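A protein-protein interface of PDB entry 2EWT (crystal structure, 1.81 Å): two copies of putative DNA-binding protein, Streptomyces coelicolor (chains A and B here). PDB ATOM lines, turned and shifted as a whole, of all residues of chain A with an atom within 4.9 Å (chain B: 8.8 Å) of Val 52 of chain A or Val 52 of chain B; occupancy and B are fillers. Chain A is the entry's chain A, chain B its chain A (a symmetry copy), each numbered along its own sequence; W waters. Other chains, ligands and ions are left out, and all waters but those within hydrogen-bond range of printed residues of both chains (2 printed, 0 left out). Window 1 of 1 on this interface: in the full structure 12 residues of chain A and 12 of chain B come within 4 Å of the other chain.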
ATOM      1  N   MET A   1      34.980  28.607 -31.175  1.00  0.00           N
ATOM      2  CA  MET A   1      35.876  28.455 -29.989  1.00  0.00           C
ATOM      3  C   MET A   1      37.336  28.379 -30.413  1.00  0.00           C
ATOM      4  O   MET A   1      37.642  27.953 -31.526  1.00  0.00           O
ATOM      5  CB  MET A   1      35.513  27.189 -29.209  1.00  0.00           C
ATOM      6  CG  MET A   1      34.090  27.175 -28.684  1.00  0.00           C
ATOM      7  SD  MET A   1      33.771  25.768 -27.610  1.00  0.00           S
ATOM      8  CE  MET A   1      33.145  24.557 -28.796  1.00  0.00           C
ATOM      9  N   TYR A   5      40.825  25.637 -26.789  1.00  0.00           N
ATOM     10  CA  TYR A   5      39.639  25.283 -26.018  1.00  0.00           C
ATOM     11  C   TYR A   5      38.954  24.053 -26.612  1.00  0.00           C
ATOM     12  O   TYR A   5      38.578  23.130 -25.885  1.00  0.00           O
ATOM     13  CB  TYR A   5      38.633  26.435 -25.974  1.00  0.00           C
ATOM     14  CG  TYR A   5      37.584  26.253 -24.898  1.00  0.00           C
ATOM     15  CD1 TYR A   5      37.794  26.733 -23.605  1.00  0.00           C
ATOM     16  CD2 TYR A   5      36.398  25.563 -25.157  1.00  0.00           C
ATOM     17  CE1 TYR A   5      36.853  26.535 -22.599  1.00  0.00           C
ATOM     18  CE2 TYR A   5      35.452  25.358 -24.154  1.00  0.00           C
ATOM     19  CZ  TYR A   5      35.682  25.845 -22.881  1.00  0.00           C
ATOM     20  OH  TYR A   5      34.744  25.651 -21.892  1.00  0.00           O
ATOM     21  N   LEU A   9      38.479  20.545 -24.705  1.00  0.00           N
ATOM     22  CA  LEU A   9      37.117  20.078 -24.463  1.00  0.00           C
ATOM     23  C   LEU A   9      37.000  18.667 -25.037  1.00  0.00           C
ATOM     24  O   LEU A   9      36.429  17.769 -24.410  1.00  0.00           O
ATOM     25  CB  LEU A   9      36.106  21.009 -25.143  1.00  0.00           C
ATOM     26  CG  LEU A   9      34.633  20.579 -25.154  1.00  0.00           C
ATOM     27  CD1 LEU A   9      34.102  20.483 -23.724  1.00  0.00           C
ATOM     28  CD2 LEU A   9      33.817  21.577 -25.962  1.00  0.00           C
ATOM     29  N   VAL A  50      31.266  21.600 -30.886  1.00  0.00           N
ATOM     30  CA  VAL A  50      30.371  20.995 -29.908  1.00  0.00           C
ATOM     31  C   VAL A  50      29.547  22.145 -29.324  1.00  0.00           C
ATOM     32  O   VAL A  50      30.099  23.016 -28.659  1.00  0.00           O
ATOM     33  CB  VAL A  50      31.162  20.326 -28.754  1.00  0.00           C
ATOM     34  CG1 VAL A  50      30.203  19.846 -27.672  1.00  0.00           C
ATOM     35  CG2 VAL A  50      31.980  19.162 -29.283  1.00  0.00           C
ATOM     36  N   THR A  51      28.242  22.159 -29.587  1.00  0.00           N
ATOM     37  CA  THR A  51      27.377  23.220 -29.067  1.00  0.00           C
ATOM     38  C   THR A  51      27.093  22.992 -27.589  1.00  0.00           C
ATOM     39  O   THR A  51      27.312  21.902 -27.069  1.00  0.00           O
ATOM     40  CB  THR A  51      26.014  23.262 -29.791  1.00  0.00           C
ATOM     41  OG1 THR A  51      25.273  22.073 -29.483  1.00  0.00           O
ATOM     42  CG2 THR A  51      26.208  23.361 -31.295  1.00  0.00           C
ATOM     43  N   VAL A  52      26.605  24.023 -26.909  1.00  0.00           N
ATOM     44  CA  VAL A  52      26.282  23.871 -25.496  1.00  0.00           C
ATOM     45  C   VAL A  52      25.225  22.772 -25.348  1.00  0.00           C
ATOM     46  O   VAL A  52      25.335  21.898 -24.490  1.00  0.00           O
ATOM     47  CB  VAL A  52      25.724  25.180 -24.898  1.00  0.00           C
ATOM     48  CG1 VAL A  52      25.202  24.924 -23.492  1.00  0.00           C
ATOM     49  CG2 VAL A  52      26.821  26.243 -24.858  1.00  0.00           C
ATOM     50  N   GLN A  53      24.202  22.817 -26.195  1.00  0.00           N
ATOM     51  CA  GLN A  53      23.134  21.818 -26.133  1.00  0.00           C
ATOM     52  C   GLN A  53      23.697  20.406 -26.299  1.00  0.00           C
ATOM     53  O   GLN A  53      23.345  19.498 -25.544  1.00  0.00           O
ATOM     54  CB  GLN A  53      22.077  22.110 -27.205  1.00  0.00           C
ATOM     55  CG  GLN A  53      20.918  21.119 -27.240  1.00  0.00           C
ATOM     56  CD  GLN A  53      19.801  21.563 -28.168  1.00  0.00           C
ATOM     57  OE1 GLN A  53      20.050  22.144 -29.221  1.00  0.00           O
ATOM     58  NE2 GLN A  53      18.563  21.276 -27.786  1.00  0.00           N
ATOM     59  N   ARG A  54      24.588  20.229 -27.271  1.00  0.00           N
ATOM     60  CA  ARG A  54      25.196  18.923 -27.516  1.00  0.00           C
ATOM     61  C   ARG A  54      26.053  18.501 -26.321  1.00  0.00           C
ATOM     62  O   ARG A  54      26.028  17.341 -25.910  1.00  0.00           O
ATOM     63  CB  ARG A  54      26.068  18.965 -28.776  1.00  0.00           C
ATOM     64  CG  ARG A  54      26.476  17.589 -29.292  1.00  0.00           C
ATOM     65  CD  ARG A  54      25.270  16.836 -29.846  1.00  0.00           C
ATOM     66  NE  ARG A  54      24.761  17.454 -31.070  1.00  0.00           N
ATOM     67  CZ  ARG A  54      23.601  17.145 -31.643  1.00  0.00           C
ATOM     68  NH1 ARG A  54      22.814  16.223 -31.105  1.00  0.00           N
ATOM     69  NH2 ARG A  54      23.229  17.756 -32.760  1.00  0.00           N
ATOM     70  N   LEU A  55      26.819  19.439 -25.766  1.00  0.00           N
ATOM     71  CA  LEU A  55      27.661  19.114 -24.616  1.00  0.00           C
ATOM     72  C   LEU A  55      26.806  18.636 -23.446  1.00  0.00           C
ATOM     73  O   LEU A  55      27.153  17.671 -22.763  1.00  0.00           O
ATOM     74  CB  LEU A  55      28.491  20.325 -24.183  1.00  0.00           C
ATOM     75  CG  LEU A  55      29.500  20.032 -23.064  1.00  0.00           C
ATOM     76  CD1 LEU A  55      30.470  18.954 -23.529  1.00  0.00           C
ATOM     77  CD2 LEU A  55      30.251  21.298 -22.685  1.00  0.00           C
ATOM     78  N   ALA A  56      25.687  19.317 -23.216  1.00  0.00           N
ATOM     79  CA  ALA A  56      24.787  18.948 -22.131  1.00  0.00           C
ATOM     80  C   ALA A  56      24.198  17.560 -22.370  1.00  0.00           C
ATOM     81  O   ALA A  56      24.039  16.778 -21.435  1.00  0.00           O
ATOM     82  CB  ALA A  56      23.667  19.979 -22.003  1.00  0.00           C
ATOM     83  N   LEU A  70      34.366  20.462 -18.944  1.00  0.00           N
ATOM     84  CA  LEU A  70      34.873  21.793 -19.273  1.00  0.00           C
ATOM     85  C   LEU A  70      36.376  21.962 -19.046  1.00  0.00           C
ATOM     86  O   LEU A  70      36.894  21.611 -17.986  1.00  0.00           O
ATOM     87  CB  LEU A  70      34.117  22.856 -18.463  1.00  0.00           C
ATOM     88  CG  LEU A  70      32.624  23.022 -18.762  1.00  0.00           C
ATOM     89  CD1 LEU A  70      32.049  24.125 -17.891  1.00  0.00           C
ATOM     90  CD2 LEU A  70      32.426  23.351 -20.233  1.00  0.00           C
ATOM     91  N   MET B   1      22.204  25.249 -32.260  1.00  0.00           N
ATOM     92  CA  MET B   1      21.270  24.811 -31.179  1.00  0.00           C
ATOM     93  C   MET B   1      19.824  25.096 -31.558  1.00  0.00           C
ATOM     94  O   MET B   1      19.549  26.012 -32.331  1.00  0.00           O
ATOM     95  CB  MET B   1      21.599  25.534 -29.871  1.00  0.00           C
ATOM     96  CG  MET B   1      23.005  25.279 -29.361  1.00  0.00           C
ATOM     97  SD  MET B   1      23.279  25.982 -27.729  1.00  0.00           S
ATOM     98  CE  MET B   1      23.932  27.612 -28.155  1.00  0.00           C
ATOM     99  N   SER B   2      18.899  24.312 -31.010  1.00  0.00           N
ATOM    100  CA  SER B   2      17.486  24.504 -31.307  1.00  0.00           C
ATOM    101  C   SER B   2      17.052  25.874 -30.802  1.00  0.00           C
ATOM    102  O   SER B   2      17.635  26.406 -29.857  1.00  0.00           O
ATOM    103  CB  SER B   2      16.639  23.419 -30.635  1.00  0.00           C
ATOM    104  OG  SER B   2      16.557  23.621 -29.236  1.00  0.00           O
ATOM    105  N   TYR B   5      16.202  25.753 -27.167  1.00  0.00           N
ATOM    106  CA  TYR B   5      17.361  25.677 -26.285  1.00  0.00           C
ATOM    107  C   TYR B   5      18.054  27.035 -26.182  1.00  0.00           C
ATOM    108  O   TYR B   5      18.400  27.484 -25.087  1.00  0.00           O
ATOM    109  CB  TYR B   5      18.374  24.642 -26.777  1.00  0.00           C
ATOM    110  CG  TYR B   5      19.388  24.269 -25.716  1.00  0.00           C
ATOM    111  CD1 TYR B   5      19.142  23.221 -24.828  1.00  0.00           C
ATOM    112  CD2 TYR B   5      20.575  24.987 -25.570  1.00  0.00           C
ATOM    113  CE1 TYR B   5      20.049  22.896 -23.824  1.00  0.00           C
ATOM    114  CE2 TYR B   5      21.488  24.670 -24.564  1.00  0.00           C
ATOM    115  CZ  TYR B   5      21.223  23.626 -23.698  1.00  0.00           C
ATOM    116  OH  TYR B   5      22.128  23.307 -22.711  1.00  0.00           O
ATOM    117  N   ALA B   6      18.260  27.680 -27.327  1.00  0.00           N
ATOM    118  CA  ALA B   6      18.915  28.985 -27.367  1.00  0.00           C
ATOM    119  C   ALA B   6      18.115  30.012 -26.572  1.00  0.00           C
ATOM    120  O   ALA B   6      18.676  30.823 -25.844  1.00  0.00           O
ATOM    121  CB  ALA B   6      19.070  29.449 -28.811  1.00  0.00           C
ATOM    122  N   LEU B   9      18.441  29.166 -22.795  1.00  0.00           N
ATOM    123  CA  LEU B   9      19.790  29.445 -22.314  1.00  0.00           C
ATOM    124  C   LEU B   9      19.914  30.956 -22.124  1.00  0.00           C
ATOM    125  O   LEU B   9      20.458  31.430 -21.122  1.00  0.00           O
ATOM    126  CB  LEU B   9      20.830  28.955 -23.330  1.00  0.00           C
ATOM    127  CG  LEU B   9      22.299  29.325 -23.084  1.00  0.00           C
ATOM    128  CD1 LEU B   9      22.785  28.707 -21.773  1.00  0.00           C
ATOM    129  CD2 LEU B   9      23.148  28.840 -24.250  1.00  0.00           C
ATOM    130  N   LEU B  13      20.658  33.273 -18.742  1.00  0.00           N
ATOM    131  CA  LEU B  13      21.747  34.245 -18.736  1.00  0.00           C
ATOM    132  C   LEU B  13      21.196  35.588 -18.261  1.00  0.00           C
ATOM    133  O   LEU B  13      21.841  36.301 -17.486  1.00  0.00           O
ATOM    134  CB  LEU B  13      22.343  34.395 -20.142  1.00  0.00           C
ATOM    135  CG  LEU B  13      23.430  33.379 -20.515  1.00  0.00           C
ATOM    136  CD1 LEU B  13      23.715  33.438 -22.010  1.00  0.00           C
ATOM    137  CD2 LEU B  13      24.688  33.676 -19.722  1.00  0.00           C
ATOM    138  N   ALA B  49      24.632  32.931 -31.341  1.00  0.00           N
ATOM    139  CA  ALA B  49      25.128  31.698 -30.733  1.00  0.00           C
ATOM    140  C   ALA B  49      26.106  31.898 -29.581  1.00  0.00           C
ATOM    141  O   ALA B  49      27.064  32.663 -29.684  1.00  0.00           O
ATOM    142  CB  ALA B  49      25.771  30.818 -31.800  1.00  0.00           C
ATOM    143  N   VAL B  50      25.851  31.197 -28.480  1.00  0.00           N
ATOM    144  CA  VAL B  50      26.710  31.243 -27.304  1.00  0.00           C
ATOM    145  C   VAL B  50      27.524  29.947 -27.329  1.00  0.00           C
ATOM    146  O   VAL B  50      26.959  28.866 -27.189  1.00  0.00           O
ATOM    147  CB  VAL B  50      25.878  31.270 -25.995  1.00  0.00           C
ATOM    148  CG1 VAL B  50      26.799  31.155 -24.787  1.00  0.00           C
ATOM    149  CG2 VAL B  50      25.068  32.551 -25.915  1.00  0.00           C
ATOM    150  N   THR B  51      28.837  30.052 -27.525  1.00  0.00           N
ATOM    151  CA  THR B  51      29.694  28.865 -27.561  1.00  0.00           C
ATOM    152  C   THR B  51      29.931  28.342 -26.151  1.00  0.00           C
ATOM    153  O   THR B  51      29.686  29.043 -25.173  1.00  0.00           O
ATOM    154  CB  THR B  51      31.079  29.170 -28.170  1.00  0.00           C
ATOM    155  OG1 THR B  51      31.801  30.053 -27.299  1.00  0.00           O
ATOM    156  CG2 THR B  51      30.933  29.818 -29.537  1.00  0.00           C
ATOM    157  N   VAL B  52      30.405  27.106 -26.044  1.00  0.00           N
ATOM    158  CA  VAL B  52      30.683  26.548 -24.727  1.00  0.00           C
ATOM    159  C   VAL B  52      31.726  27.427 -24.030  1.00  0.00           C
ATOM    160  O   VAL B  52      31.582  27.773 -22.858  1.00  0.00           O
ATOM    161  CB  VAL B  52      31.233  25.110 -24.825  1.00  0.00           C
ATOM    162  CG1 VAL B  52      31.709  24.644 -23.457  1.00  0.00           C
ATOM    163  CG2 VAL B  52      30.144  24.171 -25.342  1.00  0.00           C
ATOM    164  N   GLN B  53      32.775  27.792 -24.759  1.00  0.00           N
ATOM    165  CA  GLN B  53      33.832  28.626 -24.185  1.00  0.00           C
ATOM    166  C   GLN B  53      33.264  29.944 -23.660  1.00  0.00           C
ATOM    167  O   GLN B  53      33.585  30.367 -22.547  1.00  0.00           O
ATOM    168  CB  GLN B  53      34.925  28.885 -25.230  1.00  0.00           C
ATOM    169  CG  GLN B  53      36.077  29.758 -24.741  1.00  0.00           C
ATOM    170  CD  GLN B  53      37.225  29.813 -25.733  1.00  0.00           C
ATOM    171  OE1 GLN B  53      37.013  29.820 -26.943  1.00  0.00           O
ATOM    172  NE2 GLN B  53      38.448  29.867 -25.221  1.00  0.00           N
ATOM    173  N   ARG B  54      32.402  30.579 -24.449  1.00  0.00           N
ATOM    174  CA  ARG B  54      31.791  31.844 -24.046  1.00  0.00           C
ATOM    175  C   ARG B  54      30.894  31.638 -22.824  1.00  0.00           C
ATOM    176  O   ARG B  54      30.897  32.451 -21.899  1.00  0.00           O
ATOM    177  CB  ARG B  54      30.959  32.429 -25.193  1.00  0.00           C
ATOM    178  CG  ARG B  54      30.556  33.885 -24.986  1.00  0.00           C
ATOM    179  CD  ARG B  54      31.773  34.803 -25.065  1.00  0.00           C
ATOM    180  NE  ARG B  54      32.325  34.856 -26.419  1.00  0.00           N
ATOM    181  CZ  ARG B  54      33.499  35.394 -26.732  1.00  0.00           C
ATOM    182  NH1 ARG B  54      34.262  35.932 -25.789  1.00  0.00           N
ATOM    183  NH2 ARG B  54      33.911  35.403 -27.994  1.00  0.00           N
ATOM    184  N   LEU B  55      30.119  30.555 -22.820  1.00  0.00           N
ATOM    185  CA  LEU B  55      29.239  30.286 -21.684  1.00  0.00           C
ATOM    186  C   LEU B  55      30.054  30.126 -20.404  1.00  0.00           C
ATOM    187  O   LEU B  55      29.677  30.638 -19.348  1.00  0.00           O
ATOM    188  CB  LEU B  55      28.406  29.024 -21.922  1.00  0.00           C
ATOM    189  CG  LEU B  55      27.360  28.742 -20.834  1.00  0.00           C
ATOM    190  CD1 LEU B  55      26.397  29.919 -20.745  1.00  0.00           C
ATOM    191  CD2 LEU B  55      26.608  27.458 -21.143  1.00  0.00           C
ATOM    192  N   ALA B  56      31.170  29.410 -20.500  1.00  0.00           N
ATOM    193  CA  ALA B  56      32.033  29.196 -19.345  1.00  0.00           C
ATOM    194  C   ALA B  56      32.618  30.520 -18.860  1.00  0.00           C
ATOM    195  O   ALA B  56      32.742  30.747 -17.657  1.00  0.00           O
ATOM    196  CB  ALA B  56      33.157  28.225 -19.701  1.00  0.00           C
ATOM    197  N   GLU B  57      32.975  31.393 -19.797  1.00  0.00           N
ATOM    198  CA  GLU B  57      33.546  32.691 -19.445  1.00  0.00           C
ATOM    199  C   GLU B  57      32.500  33.563 -18.755  1.00  0.00           C
ATOM    200  O   GLU B  57      32.806  34.271 -17.794  1.00  0.00           O
ATOM    201  CB  GLU B  57      34.083  33.391 -20.700  1.00  0.00           C
ATOM    202  CG  GLU B  57      35.093  32.542 -21.471  1.00  0.00           C
ATOM    203  CD  GLU B  57      35.545  33.163 -22.781  1.00  0.00           C
ATOM    204  OE1 GLU B  57      34.703  33.741 -23.501  1.00  0.00           O
ATOM    205  OE2 GLU B  57      36.747  33.050 -23.101  1.00  0.00           O
ATOM    206  N   LEU B  58      31.262  33.506 -19.239  1.00  0.00           N
ATOM    207  CA  LEU B  58      30.188  34.293 -18.645  1.00  0.00           C
ATOM    208  C   LEU B  58      29.819  33.763 -17.266  1.00  0.00           C
ATOM    209  O   LEU B  58      29.516  34.540 -16.360  1.00  0.00           O
ATOM    210  CB  LEU B  58      28.958  34.284 -19.554  1.00  0.00           C
ATOM    211  CG  LEU B  58      29.147  35.039 -20.872  1.00  0.00           C
ATOM    212  CD1 LEU B  58      27.935  34.822 -21.768  1.00  0.00           C
ATOM    213  CD2 LEU B  58      29.350  36.533 -20.590  1.00  0.00           C
ATOM    214  N   ALA B  59      29.849  32.443 -17.105  1.00  0.00           N
ATOM    215  CA  ALA B  59      29.529  31.835 -15.816  1.00  0.00           C
ATOM    216  C   ALA B  59      30.512  32.342 -14.772  1.00  0.00           C
ATOM    217  O   ALA B  59      30.120  32.713 -13.663  1.00  0.00           O
ATOM    218  CB  ALA B  59      29.610  30.316 -15.911  1.00  0.00           C
ATOM    219  N   ASP B  60      31.793  32.352 -15.136  1.00  0.00           N
ATOM    220  CA  ASP B  60      32.850  32.820 -14.244  1.00  0.00           C
ATOM    221  C   ASP B  60      32.632  34.289 -13.909  1.00  0.00           C
ATOM    222  O   ASP B  60      32.739  34.697 -12.751  1.00  0.00           O
ATOM    223  CB  ASP B  60      34.215  32.641 -14.910  1.00  0.00           C
ATOM    224  CG  ASP B  60      34.632  31.186 -15.003  1.00  0.00           C
ATOM    225  OD1 ASP B  60      33.749  30.309 -14.909  1.00  0.00           O
ATOM    226  OD2 ASP B  60      35.838  30.919 -15.179  1.00  0.00           O
ATOM    227  N   VAL B  66      28.421  26.773 -14.311  1.00  0.00           N
ATOM    228  CA  VAL B  66      27.825  26.676 -15.641  1.00  0.00           C
ATOM    229  C   VAL B  66      26.443  26.025 -15.565  1.00  0.00           C
ATOM    230  O   VAL B  66      25.521  26.423 -16.271  1.00  0.00           O
ATOM    231  CB  VAL B  66      28.720  25.852 -16.602  1.00  0.00           C
ATOM    232  CG1 VAL B  66      28.946  24.461 -16.041  1.00  0.00           C
ATOM    233  CG2 VAL B  66      28.076  25.767 -17.976  1.00  0.00           C
ATOM    234  N   LEU B  69      23.249  28.000 -15.567  1.00  0.00           N
ATOM    235  CA  LEU B  69      22.854  28.655 -16.808  1.00  0.00           C
ATOM    236  C   LEU B  69      22.286  27.700 -17.857  1.00  0.00           C
ATOM    237  O   LEU B  69      21.766  28.142 -18.881  1.00  0.00           O
ATOM    238  CB  LEU B  69      24.057  29.398 -17.397  1.00  0.00           C
ATOM    239  CG  LEU B  69      24.725  30.456 -16.515  1.00  0.00           C
ATOM    240  CD1 LEU B  69      25.970  30.984 -17.212  1.00  0.00           C
ATOM    241  CD2 LEU B  69      23.745  31.591 -16.229  1.00  0.00           C
ATOM    242  N   LEU B  70      22.372  26.399 -17.599  1.00  0.00           N
ATOM    243  CA  LEU B  70      21.886  25.401 -18.549  1.00  0.00           C
ATOM    244  C   LEU B  70      20.379  25.155 -18.481  1.00  0.00           C
ATOM    245  O   LEU B  70      19.825  24.949 -17.401  1.00  0.00           O
ATOM    246  CB  LEU B  70      22.625  24.073 -18.337  1.00  0.00           C
ATOM    247  CG  LEU B  70      24.129  24.061 -18.632  1.00  0.00           C
ATOM    248  CD1 LEU B  70      24.685  22.669 -18.392  1.00  0.00           C
ATOM    249  CD2 LEU B  70      24.375  24.488 -20.070  1.00  0.00           C
ATOM    250  N   PRO B  71      19.698  25.170 -19.644  1.00  0.00           N
ATOM    251  CA  PRO B  71      18.251  24.943 -19.709  1.00  0.00           C
ATOM    252  C   PRO B  71      17.860  23.610 -19.075  1.00  0.00           C
ATOM    253  O   PRO B  71      18.719  22.701 -19.049  1.00  0.00           O
ATOM    254  CB  PRO B  71      17.969  24.953 -21.211  1.00  0.00           C
ATOM    255  CG  PRO B  71      18.999  25.902 -21.741  1.00  0.00           C
ATOM    256  CD  PRO B  71      20.237  25.492 -20.980  1.00  0.00           C
ATOM    257  OXT PRO B  71      16.694  23.482 -18.633  1.00  0.00           O
HETATM  258  O   HOH W   1      27.082  26.482 -28.596  1.00  0.00           O
HETATM  259  O   HOH W   2      30.001  25.785 -28.729  1.00  0.00           O
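Water W1 lies within hydrogen-bond range of O of Val 50 of chain B (2.8 Å) and N of Val 52 of chain A (3.0 Å). Water W2 bridges O of Val 50 of chain A and N of Val 52 of chain B.
Val 52 of chain B touches seven residues of chain A. Of chain B, only Met 1 and Val 52 come within 4 Å of Thr 51 of chain A. Printed residues of chain A within 4 Å of Gln 53 of chain B: Met 1 (3.5 Å) and Tyr 5 (3.5 Å). Printed residues of chain A within 4 Å of Leu 70 of chain B: Val 52 (3.5 Å). The nearest residue of chain B that does not touch Val 52 of chain A is Leu 9 of chain B (4.5 Å). The nearest printed residue of chain A that does not touch Leu 70 of chain B is Ala 56 of chain A (4.6 Å).
SD of Met 1 of chain A is in hydrogen-bond range of N of Gln 53 of chain B, 3.6 Å away. The backbone NH of Gln 53 of chain A lies within hydrogen-bond range of the side-chain sulfur of Met 1 of chain B. The backbone NH (N) of Ser 2 of chain B sits at hydrogen-bond distance from the side-chain amide oxygen (OE1) of Gln 53 of chain A (3.0 Å).
OG of Ser 2 of chain B is in hydrogen-bond range of N of Tyr 5 of chain B, 3.0 Å away. The backbone NH (N) of Arg 54 of chain A lies within hydrogen-bond range of the side-chain hydroxyl (OG1) of Thr 51 of chain A, at 3.0 Å. The side-chain hydroxyl (OG1) of Thr 51 of chain B is in hydrogen-bond range of the backbone NH (N) of Arg 54 of chain B.
Printed residues of chain B that touch a printed residue of chain A: Met 1, Ser 2, Tyr 5, Val 50, Thr 51, Val 52, Gln 53, Leu 55, Ala 56, Val 66 and Leu 70. Along chain B the printed residues that touch a printed residue of chain A span positions 1 to 70. Hydrophobic or aromatic side chains of chain A within 4 Å of the printed part of chain B: Met 1, Tyr 5, Val 52, Leu 55, Ala 56 and Leu 70. Among the printed residues, no Asp or Glu carboxylate lies within 4 Å of a Lys or Arg side-chain nitrogen of the other chain.
Met 1 of chain A touches Thr 51 of chain B. SD of Met 1 of chain A touches CB of Val 52 of chain B, at 3.8 Å. Val 50 of chain A touches Val 52 of chain B. C of Thr 51 of chain A touches CG2 of Val 52 of chain B (3.97 Å). CG2 of Val 52 of chain A touches O of Val 50 of chain B, at 3.5 Å. N of Val 52 of chain B touches CG2 of Val 52 of chain A (3.9 Å). Val 52 of chain A touches Leu 70 of chain B (CG1 to CD2, 3.5 Å). Val 52 of chain B touches Leu 55 of chain A. Tyr 5 of chain B touches Ala 56 of chain A. CG1 of Val 52 of chain B touches CD2 of Leu 70 of chain A (3.5 Å).
Met 1 of chain A touches Thr 51 of chain B, and with the chains exchanged Thr 51 of chain A touches Met 1 of chain B. Tyr 5 of chain A touches Ala 56 of chain B, and with the chains exchanged Ala 56 of chain A touches Tyr 5 of chain B. Thr 51 of chain A touches Val 52 of chain B, and with the chains exchanged Val 52 of chain A touches Thr 51 of chain B. Val 52 of chain A touches Leu 55 of chain B, and with the chains exchanged Leu 55 of chain A touches Val 52 of chain B. 11 positions are printed for both chains. Of the 23 pairs that touch across the chains among the printed residues, 21 have their exchanged pair printed and touching as well.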
